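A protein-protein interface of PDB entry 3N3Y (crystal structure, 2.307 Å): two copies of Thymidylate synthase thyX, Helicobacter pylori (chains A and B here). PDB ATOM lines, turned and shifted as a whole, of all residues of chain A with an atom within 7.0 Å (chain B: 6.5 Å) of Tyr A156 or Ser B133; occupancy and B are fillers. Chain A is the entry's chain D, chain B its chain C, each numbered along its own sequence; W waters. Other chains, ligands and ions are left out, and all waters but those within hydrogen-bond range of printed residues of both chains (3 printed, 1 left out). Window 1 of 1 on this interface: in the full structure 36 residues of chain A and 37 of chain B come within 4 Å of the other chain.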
ATOM      1  N   LEU A  97      -1.955   4.343   0.713  1.00  0.00           N
ATOM      2  CA  LEU A  97      -2.622   3.443  -0.236  1.00  0.00           C
ATOM      3  C   LEU A  97      -4.142   3.665  -0.259  1.00  0.00           C
ATOM      4  O   LEU A  97      -4.800   3.334  -1.234  1.00  0.00           O
ATOM      5  CB  LEU A  97      -2.277   1.966   0.023  1.00  0.00           C
ATOM      6  CG  LEU A  97      -1.001   1.461  -0.653  1.00  0.00           C
ATOM      7  CD1 LEU A  97      -0.860  -0.051  -0.468  1.00  0.00           C
ATOM      8  CD2 LEU A  97      -0.989   1.835  -2.133  1.00  0.00           C
ATOM      9  N   ASN A 139      -5.890  -5.493  -9.154  1.00  0.00           N
ATOM     10  CA  ASN A 139      -5.941  -6.414  -8.019  1.00  0.00           C
ATOM     11  C   ASN A 139      -5.589  -5.734  -6.687  1.00  0.00           C
ATOM     12  O   ASN A 139      -6.123  -6.094  -5.635  1.00  0.00           O
ATOM     13  CB  ASN A 139      -5.057  -7.638  -8.262  1.00  0.00           C
ATOM     14  CG  ASN A 139      -5.673  -8.615  -9.246  1.00  0.00           C
ATOM     15  OD1 ASN A 139      -4.988  -9.492  -9.777  1.00  0.00           O
ATOM     16  ND2 ASN A 139      -6.976  -8.469  -9.495  1.00  0.00           N
ATOM     17  N   LEU A 140      -4.699  -4.744  -6.731  1.00  0.00           N
ATOM     18  CA  LEU A 140      -4.378  -3.974  -5.535  1.00  0.00           C
ATOM     19  C   LEU A 140      -5.610  -3.190  -5.119  1.00  0.00           C
ATOM     20  O   LEU A 140      -6.002  -3.186  -3.948  1.00  0.00           O
ATOM     21  CB  LEU A 140      -3.191  -3.031  -5.784  1.00  0.00           C
ATOM     22  CG  LEU A 140      -2.715  -2.150  -4.621  1.00  0.00           C
ATOM     23  CD1 LEU A 140      -2.316  -2.999  -3.420  1.00  0.00           C
ATOM     24  CD2 LEU A 140      -1.557  -1.268  -5.049  1.00  0.00           C
ATOM     25  N   LEU A 143      -8.144  -5.472  -3.428  1.00  0.00           N
ATOM     26  CA  LEU A 143      -7.806  -5.791  -2.040  1.00  0.00           C
ATOM     27  C   LEU A 143      -8.148  -4.647  -1.078  1.00  0.00           C
ATOM     28  O   LEU A 143      -8.565  -4.874   0.063  1.00  0.00           O
ATOM     29  CB  LEU A 143      -6.324  -6.138  -1.915  1.00  0.00           C
ATOM     30  CG  LEU A 143      -5.837  -7.430  -2.566  1.00  0.00           C
ATOM     31  CD1 LEU A 143      -4.315  -7.457  -2.582  1.00  0.00           C
ATOM     32  CD2 LEU A 143      -6.403  -8.643  -1.847  1.00  0.00           C
ATOM     33  N   ASN A 151      -3.316  -1.574   4.703  1.00  0.00           N
ATOM     34  CA  ASN A 151      -2.223  -1.107   3.860  1.00  0.00           C
ATOM     35  C   ASN A 151      -0.983  -1.999   4.005  1.00  0.00           C
ATOM     36  O   ASN A 151      -0.354  -2.361   3.005  1.00  0.00           O
ATOM     37  CB  ASN A 151      -1.861   0.343   4.196  1.00  0.00           C
ATOM     38  CG  ASN A 151      -2.844   1.354   3.617  1.00  0.00           C
ATOM     39  OD1 ASN A 151      -3.756   0.999   2.872  1.00  0.00           O
ATOM     40  ND2 ASN A 151      -2.649   2.629   3.952  1.00  0.00           N
ATOM     41  N   ASP A 152      -0.657  -2.363   5.246  1.00  0.00           N
ATOM     42  CA  ASP A 152       0.575  -3.094   5.544  1.00  0.00           C
ATOM     43  C   ASP A 152       0.590  -4.473   4.916  1.00  0.00           C
ATOM     44  O   ASP A 152       1.654  -5.093   4.774  1.00  0.00           O
ATOM     45  CB  ASP A 152       0.803  -3.223   7.060  1.00  0.00           C
ATOM     46  CG  ASP A 152       1.504  -2.000   7.668  1.00  0.00           C
ATOM     47  OD1 ASP A 152       1.665  -0.969   6.961  1.00  0.00           O
ATOM     48  OD2 ASP A 152       1.890  -2.078   8.866  1.00  0.00           O
ATOM     49  N   LEU A 153      -0.589  -4.958   4.546  1.00  0.00           N
ATOM     50  CA  LEU A 153      -0.701  -6.266   3.915  1.00  0.00           C
ATOM     51  C   LEU A 153      -0.868  -6.150   2.409  1.00  0.00           C
ATOM     52  O   LEU A 153      -0.155  -6.798   1.647  1.00  0.00           O
ATOM     53  CB  LEU A 153      -1.870  -7.043   4.507  1.00  0.00           C
ATOM     54  CG  LEU A 153      -1.709  -7.385   5.987  1.00  0.00           C
ATOM     55  CD1 LEU A 153      -2.999  -8.000   6.507  1.00  0.00           C
ATOM     56  CD2 LEU A 153      -0.536  -8.330   6.185  1.00  0.00           C
ATOM     57  N   ALA A 154      -1.806  -5.315   1.984  1.00  0.00           N
ATOM     58  CA  ALA A 154      -2.093  -5.170   0.563  1.00  0.00           C
ATOM     59  C   ALA A 154      -0.890  -4.643  -0.217  1.00  0.00           C
ATOM     60  O   ALA A 154      -0.801  -4.849  -1.427  1.00  0.00           O
ATOM     61  CB  ALA A 154      -3.314  -4.274   0.348  1.00  0.00           C
ATOM     62  N   LYS A 155       0.030  -3.965   0.467  1.00  0.00           N
ATOM     63  CA  LYS A 155       1.192  -3.371  -0.196  1.00  0.00           C
ATOM     64  C   LYS A 155       2.110  -4.411  -0.839  1.00  0.00           C
ATOM     65  O   LYS A 155       2.857  -4.090  -1.756  1.00  0.00           O
ATOM     66  CB  LYS A 155       1.990  -2.503   0.783  1.00  0.00           C
ATOM     67  CG  LYS A 155       2.612  -3.272   1.943  1.00  0.00           C
ATOM     68  CD  LYS A 155       3.047  -2.321   3.036  1.00  0.00           C
ATOM     69  CE  LYS A 155       4.017  -1.262   2.507  1.00  0.00           C
ATOM     70  NZ  LYS A 155       5.227  -1.836   1.853  1.00  0.00           N
ATOM     71  N   TYR A 156       2.055  -5.650  -0.357  1.00  0.00           N
ATOM     72  CA  TYR A 156       2.844  -6.742  -0.933  1.00  0.00           C
ATOM     73  C   TYR A 156       2.452  -7.105  -2.369  1.00  0.00           C
ATOM     74  O   TYR A 156       3.227  -7.728  -3.093  1.00  0.00           O
ATOM     75  CB  TYR A 156       2.807  -7.978  -0.029  1.00  0.00           C
ATOM     76  CG  TYR A 156       3.722  -7.821   1.156  1.00  0.00           C
ATOM     77  CD1 TYR A 156       3.379  -6.991   2.215  1.00  0.00           C
ATOM     78  CD2 TYR A 156       4.951  -8.469   1.202  1.00  0.00           C
ATOM     79  CE1 TYR A 156       4.233  -6.822   3.305  1.00  0.00           C
ATOM     80  CE2 TYR A 156       5.804  -8.314   2.284  1.00  0.00           C
ATOM     81  CZ  TYR A 156       5.445  -7.487   3.332  1.00  0.00           C
ATOM     82  OH  TYR A 156       6.300  -7.328   4.409  1.00  0.00           O
ATOM     83  N   ALA A 157       1.261  -6.702  -2.791  1.00  0.00           N
ATOM     84  CA  ALA A 157       0.818  -7.007  -4.143  1.00  0.00           C
ATOM     85  C   ALA A 157       1.021  -5.807  -5.061  1.00  0.00           C
ATOM     86  O   ALA A 157       0.550  -5.779  -6.191  1.00  0.00           O
ATOM     87  CB  ALA A 157      -0.640  -7.447  -4.135  1.00  0.00           C
ATOM     88  N   MET A 158       1.732  -4.808  -4.570  1.00  0.00           N
ATOM     89  CA  MET A 158       1.930  -3.602  -5.345  1.00  0.00           C
ATOM     90  C   MET A 158       2.971  -3.861  -6.453  1.00  0.00           C
ATOM     91  O   MET A 158       3.977  -4.530  -6.213  1.00  0.00           O
ATOM     92  CB  MET A 158       2.342  -2.468  -4.394  1.00  0.00           C
ATOM     93  CG  MET A 158       2.802  -1.177  -5.054  1.00  0.00           C
ATOM     94  SD  MET A 158       2.908   0.205  -3.878  1.00  0.00           S
ATOM     95  CE  MET A 158       3.601  -0.601  -2.433  1.00  0.00           C
ATOM     96  N   PRO A 159       2.714  -3.358  -7.678  1.00  0.00           N
ATOM     97  CA  PRO A 159       3.693  -3.488  -8.760  1.00  0.00           C
ATOM     98  C   PRO A 159       4.789  -2.437  -8.598  1.00  0.00           C
ATOM     99  O   PRO A 159       4.552  -1.352  -8.068  1.00  0.00           O
ATOM    100  CB  PRO A 159       2.885  -3.155 -10.022  1.00  0.00           C
ATOM    101  CG  PRO A 159       1.545  -2.682  -9.547  1.00  0.00           C
ATOM    102  CD  PRO A 159       1.591  -2.498  -8.073  1.00  0.00           C
ATOM    103  N   SER B  73      11.644  -9.482   1.217  1.00  0.00           N
ATOM    104  CA  SER B  73      10.874  -8.914   0.106  1.00  0.00           C
ATOM    105  C   SER B  73      11.499  -7.633  -0.488  1.00  0.00           C
ATOM    106  O   SER B  73      12.232  -6.917   0.181  1.00  0.00           O
ATOM    107  CB  SER B  73       9.422  -8.664   0.516  1.00  0.00           C
ATOM    108  OG  SER B  73       9.280  -7.503   1.311  1.00  0.00           O
ATOM    109  N   GLY B  75       9.776  -5.123  -1.058  1.00  0.00           N
ATOM    110  CA  GLY B  75       9.119  -4.133  -0.220  1.00  0.00           C
ATOM    111  C   GLY B  75       9.882  -3.775   1.058  1.00  0.00           C
ATOM    112  O   GLY B  75      10.031  -2.599   1.397  1.00  0.00           O
ATOM    113  N   ALA B  76      10.349  -4.792   1.779  1.00  0.00           N
ATOM    114  CA  ALA B  76      11.164  -4.583   2.977  1.00  0.00           C
ATOM    115  C   ALA B  76      12.544  -4.028   2.611  1.00  0.00           C
ATOM    116  O   ALA B  76      13.164  -3.324   3.388  1.00  0.00           O
ATOM    117  CB  ALA B  76      11.305  -5.876   3.760  1.00  0.00           C
ATOM    118  N   LEU B 121       8.319 -15.596  -3.763  1.00  0.00           N
ATOM    119  CA  LEU B 121       7.561 -14.527  -3.127  1.00  0.00           C
ATOM    120  C   LEU B 121       7.543 -14.695  -1.627  1.00  0.00           C
ATOM    121  O   LEU B 121       7.606 -15.816  -1.127  1.00  0.00           O
ATOM    122  CB  LEU B 121       6.116 -14.504  -3.624  1.00  0.00           C
ATOM    123  CG  LEU B 121       5.846 -14.337  -5.119  1.00  0.00           C
ATOM    124  CD1 LEU B 121       4.421 -14.780  -5.419  1.00  0.00           C
ATOM    125  CD2 LEU B 121       6.108 -12.914  -5.590  1.00  0.00           C
ATOM    126  N   VAL B 122       7.462 -13.571  -0.919  1.00  0.00           N
ATOM    127  CA  VAL B 122       7.225 -13.571   0.516  1.00  0.00           C
ATOM    128  C   VAL B 122       5.709 -13.505   0.746  1.00  0.00           C
ATOM    129  O   VAL B 122       5.054 -12.573   0.267  1.00  0.00           O
ATOM    130  CB  VAL B 122       7.880 -12.335   1.194  1.00  0.00           C
ATOM    131  CG1 VAL B 122       7.526 -12.283   2.682  1.00  0.00           C
ATOM    132  CG2 VAL B 122       9.378 -12.329   0.991  1.00  0.00           C
ATOM    133  N   PHE B 123       5.151 -14.481   1.464  1.00  0.00           N
ATOM    134  CA  PHE B 123       3.717 -14.465   1.799  1.00  0.00           C
ATOM    135  C   PHE B 123       3.479 -13.799   3.148  1.00  0.00           C
ATOM    136  O   PHE B 123       4.267 -13.958   4.076  1.00  0.00           O
ATOM    137  CB  PHE B 123       3.133 -15.879   1.858  1.00  0.00           C
ATOM    138  CG  PHE B 123       2.868 -16.501   0.517  1.00  0.00           C
ATOM    139  CD1 PHE B 123       3.318 -15.905  -0.649  1.00  0.00           C
ATOM    140  CD2 PHE B 123       2.155 -17.695   0.425  1.00  0.00           C
ATOM    141  CE1 PHE B 123       3.074 -16.488  -1.887  1.00  0.00           C
ATOM    142  CE2 PHE B 123       1.902 -18.287  -0.813  1.00  0.00           C
ATOM    143  CZ  PHE B 123       2.374 -17.683  -1.971  1.00  0.00           C
ATOM    144  N   VAL B 124       2.379 -13.067   3.253  1.00  0.00           N
ATOM    145  CA  VAL B 124       2.007 -12.395   4.488  1.00  0.00           C
ATOM    146  C   VAL B 124       0.767 -13.048   5.091  1.00  0.00           C
ATOM    147  O   VAL B 124       0.258 -14.030   4.559  1.00  0.00           O
ATOM    148  CB  VAL B 124       1.756 -10.900   4.243  1.00  0.00           C
ATOM    149  CG1 VAL B 124       2.968 -10.292   3.565  1.00  0.00           C
ATOM    150  CG2 VAL B 124       0.524 -10.699   3.383  1.00  0.00           C
ATOM    151  N   LYS B 128      -5.697 -13.762   0.502  1.00  0.00           N
ATOM    152  CA  LYS B 128      -6.141 -12.971  -0.645  1.00  0.00           C
ATOM    153  C   LYS B 128      -4.995 -12.145  -1.247  1.00  0.00           C
ATOM    154  O   LYS B 128      -4.816 -12.117  -2.478  1.00  0.00           O
ATOM    155  CB  LYS B 128      -7.335 -12.095  -0.273  1.00  0.00           C
ATOM    156  CG  LYS B 128      -8.508 -12.884   0.308  1.00  0.00           C
ATOM    157  CD  LYS B 128      -9.762 -12.024   0.438  1.00  0.00           C
ATOM    158  CE  LYS B 128     -10.878 -12.780   1.157  1.00  0.00           C
ATOM    159  NZ  LYS B 128     -11.101 -14.153   0.585  1.00  0.00           N
ATOM    160  N   VAL B 129      -4.216 -11.498  -0.377  1.00  0.00           N
ATOM    161  CA  VAL B 129      -2.993 -10.809  -0.790  1.00  0.00           C
ATOM    162  C   VAL B 129      -2.027 -11.783  -1.460  1.00  0.00           C
ATOM    163  O   VAL B 129      -1.519 -11.521  -2.544  1.00  0.00           O
ATOM    164  CB  VAL B 129      -2.243 -10.143   0.400  1.00  0.00           C
ATOM    165  CG1 VAL B 129      -0.930  -9.529  -0.091  1.00  0.00           C
ATOM    166  CG2 VAL B 129      -3.104  -9.093   1.078  1.00  0.00           C
ATOM    167  N   ASN B 130      -1.778 -12.908  -0.801  1.00  0.00           N
ATOM    168  CA  ASN B 130      -0.855 -13.898  -1.324  1.00  0.00           C
ATOM    169  C   ASN B 130      -1.271 -14.383  -2.722  1.00  0.00           C
ATOM    170  O   ASN B 130      -0.423 -14.555  -3.593  1.00  0.00           O
ATOM    171  CB  ASN B 130      -0.709 -15.063  -0.335  1.00  0.00           C
ATOM    172  CG  ASN B 130       0.027 -14.661   0.942  1.00  0.00           C
ATOM    173  OD1 ASN B 130      -0.046 -15.347   1.966  1.00  0.00           O
ATOM    174  ND2 ASN B 130       0.734 -13.538   0.885  1.00  0.00           N
ATOM    175  N   ALA B 131      -2.575 -14.569  -2.941  1.00  0.00           N
ATOM    176  CA  ALA B 131      -3.085 -14.976  -4.253  1.00  0.00           C
ATOM    177  C   ALA B 131      -2.776 -13.930  -5.313  1.00  0.00           C
ATOM    178  O   ALA B 131      -2.302 -14.267  -6.395  1.00  0.00           O
ATOM    179  CB  ALA B 131      -4.604 -15.260  -4.200  1.00  0.00           C
ATOM    180  N   MET B 132      -3.050 -12.664  -4.998  1.00  0.00           N
ATOM    181  CA  MET B 132      -2.701 -11.555  -5.887  1.00  0.00           C
ATOM    182  C   MET B 132      -1.196 -11.463  -6.181  1.00  0.00           C
ATOM    183  O   MET B 132      -0.807 -11.114  -7.295  1.00  0.00           O
ATOM    184  CB  MET B 132      -3.199 -10.225  -5.322  1.00  0.00           C
ATOM    185  CG  MET B 132      -4.691 -10.192  -5.018  1.00  0.00           C
ATOM    186  SD  MET B 132      -5.759 -10.737  -6.377  1.00  0.00           S
ATOM    187  CE  MET B 132      -7.316  -9.960  -5.880  1.00  0.00           C
ATOM    188  N   SER B 133      -0.348 -11.772  -5.202  1.00  0.00           N
ATOM    189  CA  SER B 133       1.093 -11.781  -5.472  1.00  0.00           C
ATOM    190  C   SER B 133       1.409 -12.833  -6.527  1.00  0.00           C
ATOM    191  O   SER B 133       2.178 -12.581  -7.454  1.00  0.00           O
ATOM    192  CB  SER B 133       1.934 -12.017  -4.204  1.00  0.00           C
ATOM    193  OG  SER B 133       1.657 -11.041  -3.228  1.00  0.00           O
ATOM    194  N   VAL B 134       0.801 -14.007  -6.396  1.00  0.00           N
ATOM    195  CA  VAL B 134       1.020 -15.094  -7.358  1.00  0.00           C
ATOM    196  C   VAL B 134       0.516 -14.723  -8.752  1.00  0.00           C
ATOM    197  O   VAL B 134       1.156 -15.015  -9.752  1.00  0.00           O
ATOM    198  CB  VAL B 134       0.367 -16.391  -6.880  1.00  0.00           C
ATOM    199  CG1 VAL B 134       0.618 -17.537  -7.871  1.00  0.00           C
ATOM    200  CG2 VAL B 134       0.878 -16.739  -5.494  1.00  0.00           C
ATOM    201  N   LEU B 135      -0.625 -14.050  -8.810  1.00  0.00           N
ATOM    202  CA  LEU B 135      -1.148 -13.584 -10.084  1.00  0.00           C
ATOM    203  C   LEU B 135      -0.145 -12.666 -10.758  1.00  0.00           C
ATOM    204  O   LEU B 135       0.114 -12.801 -11.955  1.00  0.00           O
ATOM    205  CB  LEU B 135      -2.505 -12.888  -9.908  1.00  0.00           C
ATOM    206  CG  LEU B 135      -3.555 -13.743  -9.173  1.00  0.00           C
ATOM    207  CD1 LEU B 135      -4.929 -13.074  -9.131  1.00  0.00           C
ATOM    208  CD2 LEU B 135      -3.662 -15.115  -9.810  1.00  0.00           C
ATOM    209  N   ALA B 136       0.434 -11.741  -9.990  1.00  0.00           N
ATOM    210  CA  ALA B 136       1.413 -10.822 -10.549  1.00  0.00           C
ATOM    211  C   ALA B 136       2.696 -11.569 -10.913  1.00  0.00           C
ATOM    212  O   ALA B 136       3.328 -11.292 -11.933  1.00  0.00           O
ATOM    213  CB  ALA B 136       1.692  -9.672  -9.578  1.00  0.00           C
ATOM    214  N   LEU B 137       3.078 -12.530 -10.086  1.00  0.00           N
ATOM    215  CA  LEU B 137       4.230 -13.363 -10.423  1.00  0.00           C
ATOM    216  C   LEU B 137       4.025 -14.094 -11.752  1.00  0.00           C
ATOM    217  O   LEU B 137       4.918 -14.126 -12.590  1.00  0.00           O
ATOM    218  CB  LEU B 137       4.536 -14.378  -9.314  1.00  0.00           C
ATOM    219  CG  LEU B 137       5.638 -15.393  -9.647  1.00  0.00           C
ATOM    220  CD1 LEU B 137       6.971 -14.681  -9.777  1.00  0.00           C
ATOM    221  CD2 LEU B 137       5.716 -16.462  -8.577  1.00  0.00           C
ATOM    222  N   GLU B 138       2.843 -14.668 -11.946  1.00  0.00           N
ATOM    223  CA  GLU B 138       2.554 -15.408 -13.178  1.00  0.00           C
ATOM    224  C   GLU B 138       2.586 -14.510 -14.412  1.00  0.00           C
ATOM    225  O   GLU B 138       3.110 -14.900 -15.451  1.00  0.00           O
ATOM    226  CB  GLU B 138       1.217 -16.137 -13.068  1.00  0.00           C
ATOM    227  CG  GLU B 138       0.710 -16.703 -14.402  1.00  0.00           C
ATOM    228  CD  GLU B 138       1.472 -17.936 -14.897  1.00  0.00           C
ATOM    229  OE1 GLU B 138       2.262 -18.528 -14.135  1.00  0.00           O
ATOM    230  OE2 GLU B 138       1.258 -18.330 -16.063  1.00  0.00           O
ATOM    231  N   PRO B 159       5.816  -7.670  -8.439  1.00  0.00           N
ATOM    232  CA  PRO B 159       5.229  -7.307  -7.150  1.00  0.00           C
ATOM    233  C   PRO B 159       6.307  -7.116  -6.063  1.00  0.00           C
ATOM    234  O   PRO B 159       7.375  -7.743  -6.078  1.00  0.00           O
ATOM    235  CB  PRO B 159       4.361  -8.519  -6.825  1.00  0.00           C
ATOM    236  CG  PRO B 159       5.087  -9.660  -7.435  1.00  0.00           C
ATOM    237  CD  PRO B 159       5.862  -9.127  -8.622  1.00  0.00           C
ATOM    238  N   GLU B 160       6.005  -6.257  -5.104  1.00  0.00           N
ATOM    239  CA  GLU B 160       6.960  -5.919  -4.047  1.00  0.00           C
ATOM    240  C   GLU B 160       7.231  -7.081  -3.094  1.00  0.00           C
ATOM    241  O   GLU B 160       8.167  -7.037  -2.300  1.00  0.00           O
ATOM    242  CB  GLU B 160       6.493  -4.676  -3.289  1.00  0.00           C
ATOM    243  CG  GLU B 160       6.482  -3.420  -4.170  1.00  0.00           C
ATOM    244  CD  GLU B 160       7.380  -2.315  -3.634  1.00  0.00           C
ATOM    245  OE1 GLU B 160       7.293  -2.015  -2.421  1.00  0.00           O
ATOM    246  OE2 GLU B 160       8.166  -1.737  -4.415  1.00  0.00           O
ATOM    247  N   SER B 161       6.431  -8.137  -3.193  1.00  0.00           N
ATOM    248  CA  SER B 161       6.663  -9.315  -2.367  1.00  0.00           C
ATOM    249  C   SER B 161       7.735 -10.207  -2.985  1.00  0.00           C
ATOM    250  O   SER B 161       8.152 -11.184  -2.393  1.00  0.00           O
ATOM    251  CB  SER B 161       5.363 -10.089  -2.133  1.00  0.00           C
ATOM    252  OG  SER B 161       4.641 -10.199  -3.337  1.00  0.00           O
ATOM    253  N   TYR B 162       8.201  -9.852  -4.170  1.00  0.00           N
ATOM    254  CA  TYR B 162       9.267 -10.625  -4.794  1.00  0.00           C
ATOM    255  C   TYR B 162      10.484 -10.733  -3.883  1.00  0.00           C
ATOM    256  O   TYR B 162      10.878  -9.758  -3.237  1.00  0.00           O
ATOM    257  CB  TYR B 162       9.677 -10.004  -6.121  1.00  0.00           C
ATOM    258  CG  TYR B 162      10.376 -10.981  -7.014  1.00  0.00           C
ATOM    259  CD1 TYR B 162      11.765 -11.056  -7.042  1.00  0.00           C
ATOM    260  CD2 TYR B 162       9.644 -11.866  -7.818  1.00  0.00           C
ATOM    261  CE1 TYR B 162      12.420 -11.971  -7.857  1.00  0.00           C
ATOM    262  CE2 TYR B 162      10.287 -12.781  -8.642  1.00  0.00           C
ATOM    263  CZ  TYR B 162      11.676 -12.831  -8.655  1.00  0.00           C
ATOM    264  OH  TYR B 162      12.326 -13.735  -9.468  1.00  0.00           O
ATOM    265  N   LEU B 188       6.824  -2.033  10.003  1.00  0.00           N
ATOM    266  CA  LEU B 188       6.301  -3.125   9.197  1.00  0.00           C
ATOM    267  C   LEU B 188       6.687  -4.452   9.836  1.00  0.00           C
ATOM    268  O   LEU B 188       7.819  -4.621  10.304  1.00  0.00           O
ATOM    269  CB  LEU B 188       6.864  -3.041   7.776  1.00  0.00           C
ATOM    270  CG  LEU B 188       6.320  -3.987   6.706  1.00  0.00           C
ATOM    271  CD1 LEU B 188       4.869  -3.653   6.382  1.00  0.00           C
ATOM    272  CD2 LEU B 188       7.195  -3.918   5.447  1.00  0.00           C
ATOM    273  N   LYS B 189       5.736  -5.378   9.866  1.00  0.00           N
ATOM    274  CA  LYS B 189       5.928  -6.689  10.470  1.00  0.00           C
ATOM    275  C   LYS B 189       7.196  -7.368   9.983  1.00  0.00           C
ATOM    276  O   LYS B 189       7.969  -7.881  10.791  1.00  0.00           O
ATOM    277  CB  LYS B 189       4.728  -7.598  10.175  1.00  0.00           C
ATOM    278  CG  LYS B 189       4.853  -8.978  10.789  1.00  0.00           C
ATOM    279  CD  LYS B 189       5.166  -8.823  12.256  1.00  0.00           C
ATOM    280  CE  LYS B 189       5.436 -10.153  12.929  1.00  0.00           C
ATOM    281  NZ  LYS B 189       5.844  -9.919  14.345  1.00  0.00           N
ATOM    282  N   GLU B 190       7.401  -7.386   8.665  1.00  0.00           N
ATOM    283  CA  GLU B 190       8.566  -8.069   8.095  1.00  0.00           C
ATOM    284  C   GLU B 190       9.870  -7.488   8.644  1.00  0.00           C
ATOM    285  O   GLU B 190      10.816  -8.219   8.927  1.00  0.00           O
ATOM    286  CB  GLU B 190       8.569  -8.007   6.567  1.00  0.00           C
ATOM    287  CG  GLU B 190       9.757  -8.742   5.928  1.00  0.00           C
ATOM    288  CD  GLU B 190       9.645  -8.926   4.401  1.00  0.00           C
ATOM    289  OE1 GLU B 190       8.730  -8.337   3.767  1.00  0.00           O
ATOM    290  OE2 GLU B 190      10.491  -9.665   3.836  1.00  0.00           O
ATOM    291  N   MET B 191       9.903  -6.167   8.798  1.00  0.00           N
ATOM    292  CA  MET B 191      11.067  -5.501   9.355  1.00  0.00           C
ATOM    293  C   MET B 191      11.289  -5.890  10.823  1.00  0.00           C
ATOM    294  O   MET B 191      12.429  -6.100  11.248  1.00  0.00           O
ATOM    295  CB  MET B 191      10.951  -3.986   9.178  1.00  0.00           C
ATOM    296  CG  MET B 191      11.027  -3.570   7.726  1.00  0.00           C
ATOM    297  SD  MET B 191      12.576  -4.117   6.967  1.00  0.00           S
ATOM    298  CE  MET B 191      13.788  -3.153   7.879  1.00  0.00           C
HETATM  299  O   HOH W   1       2.611  -4.539   9.590  1.00  0.00           O
HETATM  300  O   HOH W   2       5.442  -3.460  -0.605  1.00  0.00           O
HETATM  301  O   HOH W   3       5.056  -7.446   6.838  1.00  0.00           O
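The side-chain carboxylate (OE1) of Glu B190 is in hydrogen-bond range of the side-chain hydroxyl (OH) of Tyr A156.
The backbone carbonyl oxygen (O) of Tyr A156 sits at hydrogen-bond distance from the side-chain hydroxyl (OG) of Ser B161.
SD of Met B132 lies close to OD1 of Asn A139 (3.7 Å).
The backbone NH of Glu B160 lies within hydrogen-bond range of the backbone carbonyl oxygen of Met A158 (2.9 Å).
The side-chain hydroxyl of Ser B133 is in hydrogen-bond range of the side-chain hydroxyl of Ser B161, 3.1 Å away.
The side-chain hydroxyl (OG) of Ser B73 sits at hydrogen-bond distance from the backbone NH (N) of Ala B76 (3.0 Å).
The backbone carbonyl oxygen (O) of Val B129 is in hydrogen-bond range of the side-chain hydroxyl (OG) of Ser B133, 3.3 Å away.
N of Val B122 sits at hydrogen-bond distance from O of Ser B161.
The side-chain hydroxyl (OG) of Ser B73 sits close to the backbone NH (N) of Gly B75, at 3.4 Å.
The backbone NH (N) of Val B124 sits close to the side-chain amide nitrogen (ND2) of Asn B130, at 2.9 Å.
Leu B135 touches Asn A139.
Leu B188 touches Asp A152.
CG1 of Val B129 touches O of Leu A153, at 3.3 Å.
O of Lys A155 touches CB of Glu B160 (3.99 Å).
OG of Ser B73 touches CE2 of Tyr A156, at 3.7 Å.
O of Tyr A156 touches OG of Ser B133, 3.7 Å away.
Pro B159 touches Tyr A156.
O of Tyr A156 touches N of Glu B160, at 3.7 Å.
Ala A157 touches Met B132 (CB to CB, 3.96 Å).
CA of Pro B159 touches O of Met A158 (3.2 Å).
Printed residues of chain B within 4 Å of Leu A143: Lys B128, Val B129 and Met B132.
Printed residues of chain B within 4 Å of Asp A152: Leu B188.
Ala A154 touches none of the printed residues of chain B.
Of the printed residues of chain B, Tyr A156 touches Ser B73 (3.7 Å), Val B124 (3.5 Å), Ser B133 (3.7 Å), Pro B159 (3.98 Å), Glu B160 (3.7 Å), Ser B161 (2.9 Å), Leu B188 (3.7 Å) and Glu B190 (2.7 Å).
Printed residues of chain B within 4 Å of Ala A157: Met B132.
Ser B133 touches just one residue of chain A: Tyr A156.
Of the printed residues of chain A, Leu B135 touches Asn A139 (3.6 Å).
Of the 26 printed residues of chain B, 12 touch a printed residue of chain A.
Hydrophobic or aromatic side chains of chain B within 4 Å of the printed part of chain A: Val B124, Val B129, Met B132, Leu B135, Pro B159 and Leu B188.
Among the printed residues, no Asp or Glu carboxylate lies within 4 Å of a Lys or Arg side-chain nitrogen of the other chain.
Position printed for both chains: 159.
Water W1 bridges the side-chain carboxylate (OD2) of Asp A152 (2.7 Å) and the backbone NH (N) of Lys B189 (3.2 Å).
Water W3 lies within hydrogen-bond range of the side-chain hydroxyl (OH) of Tyr A156 (2.7 Å) and the backbone NH (N) of Glu B190 (3.0 Å).
Water W2 lies within hydrogen-bond range of O of Lys A155 (2.9 Å) and OE1 of Glu B160 (3.0 Å).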
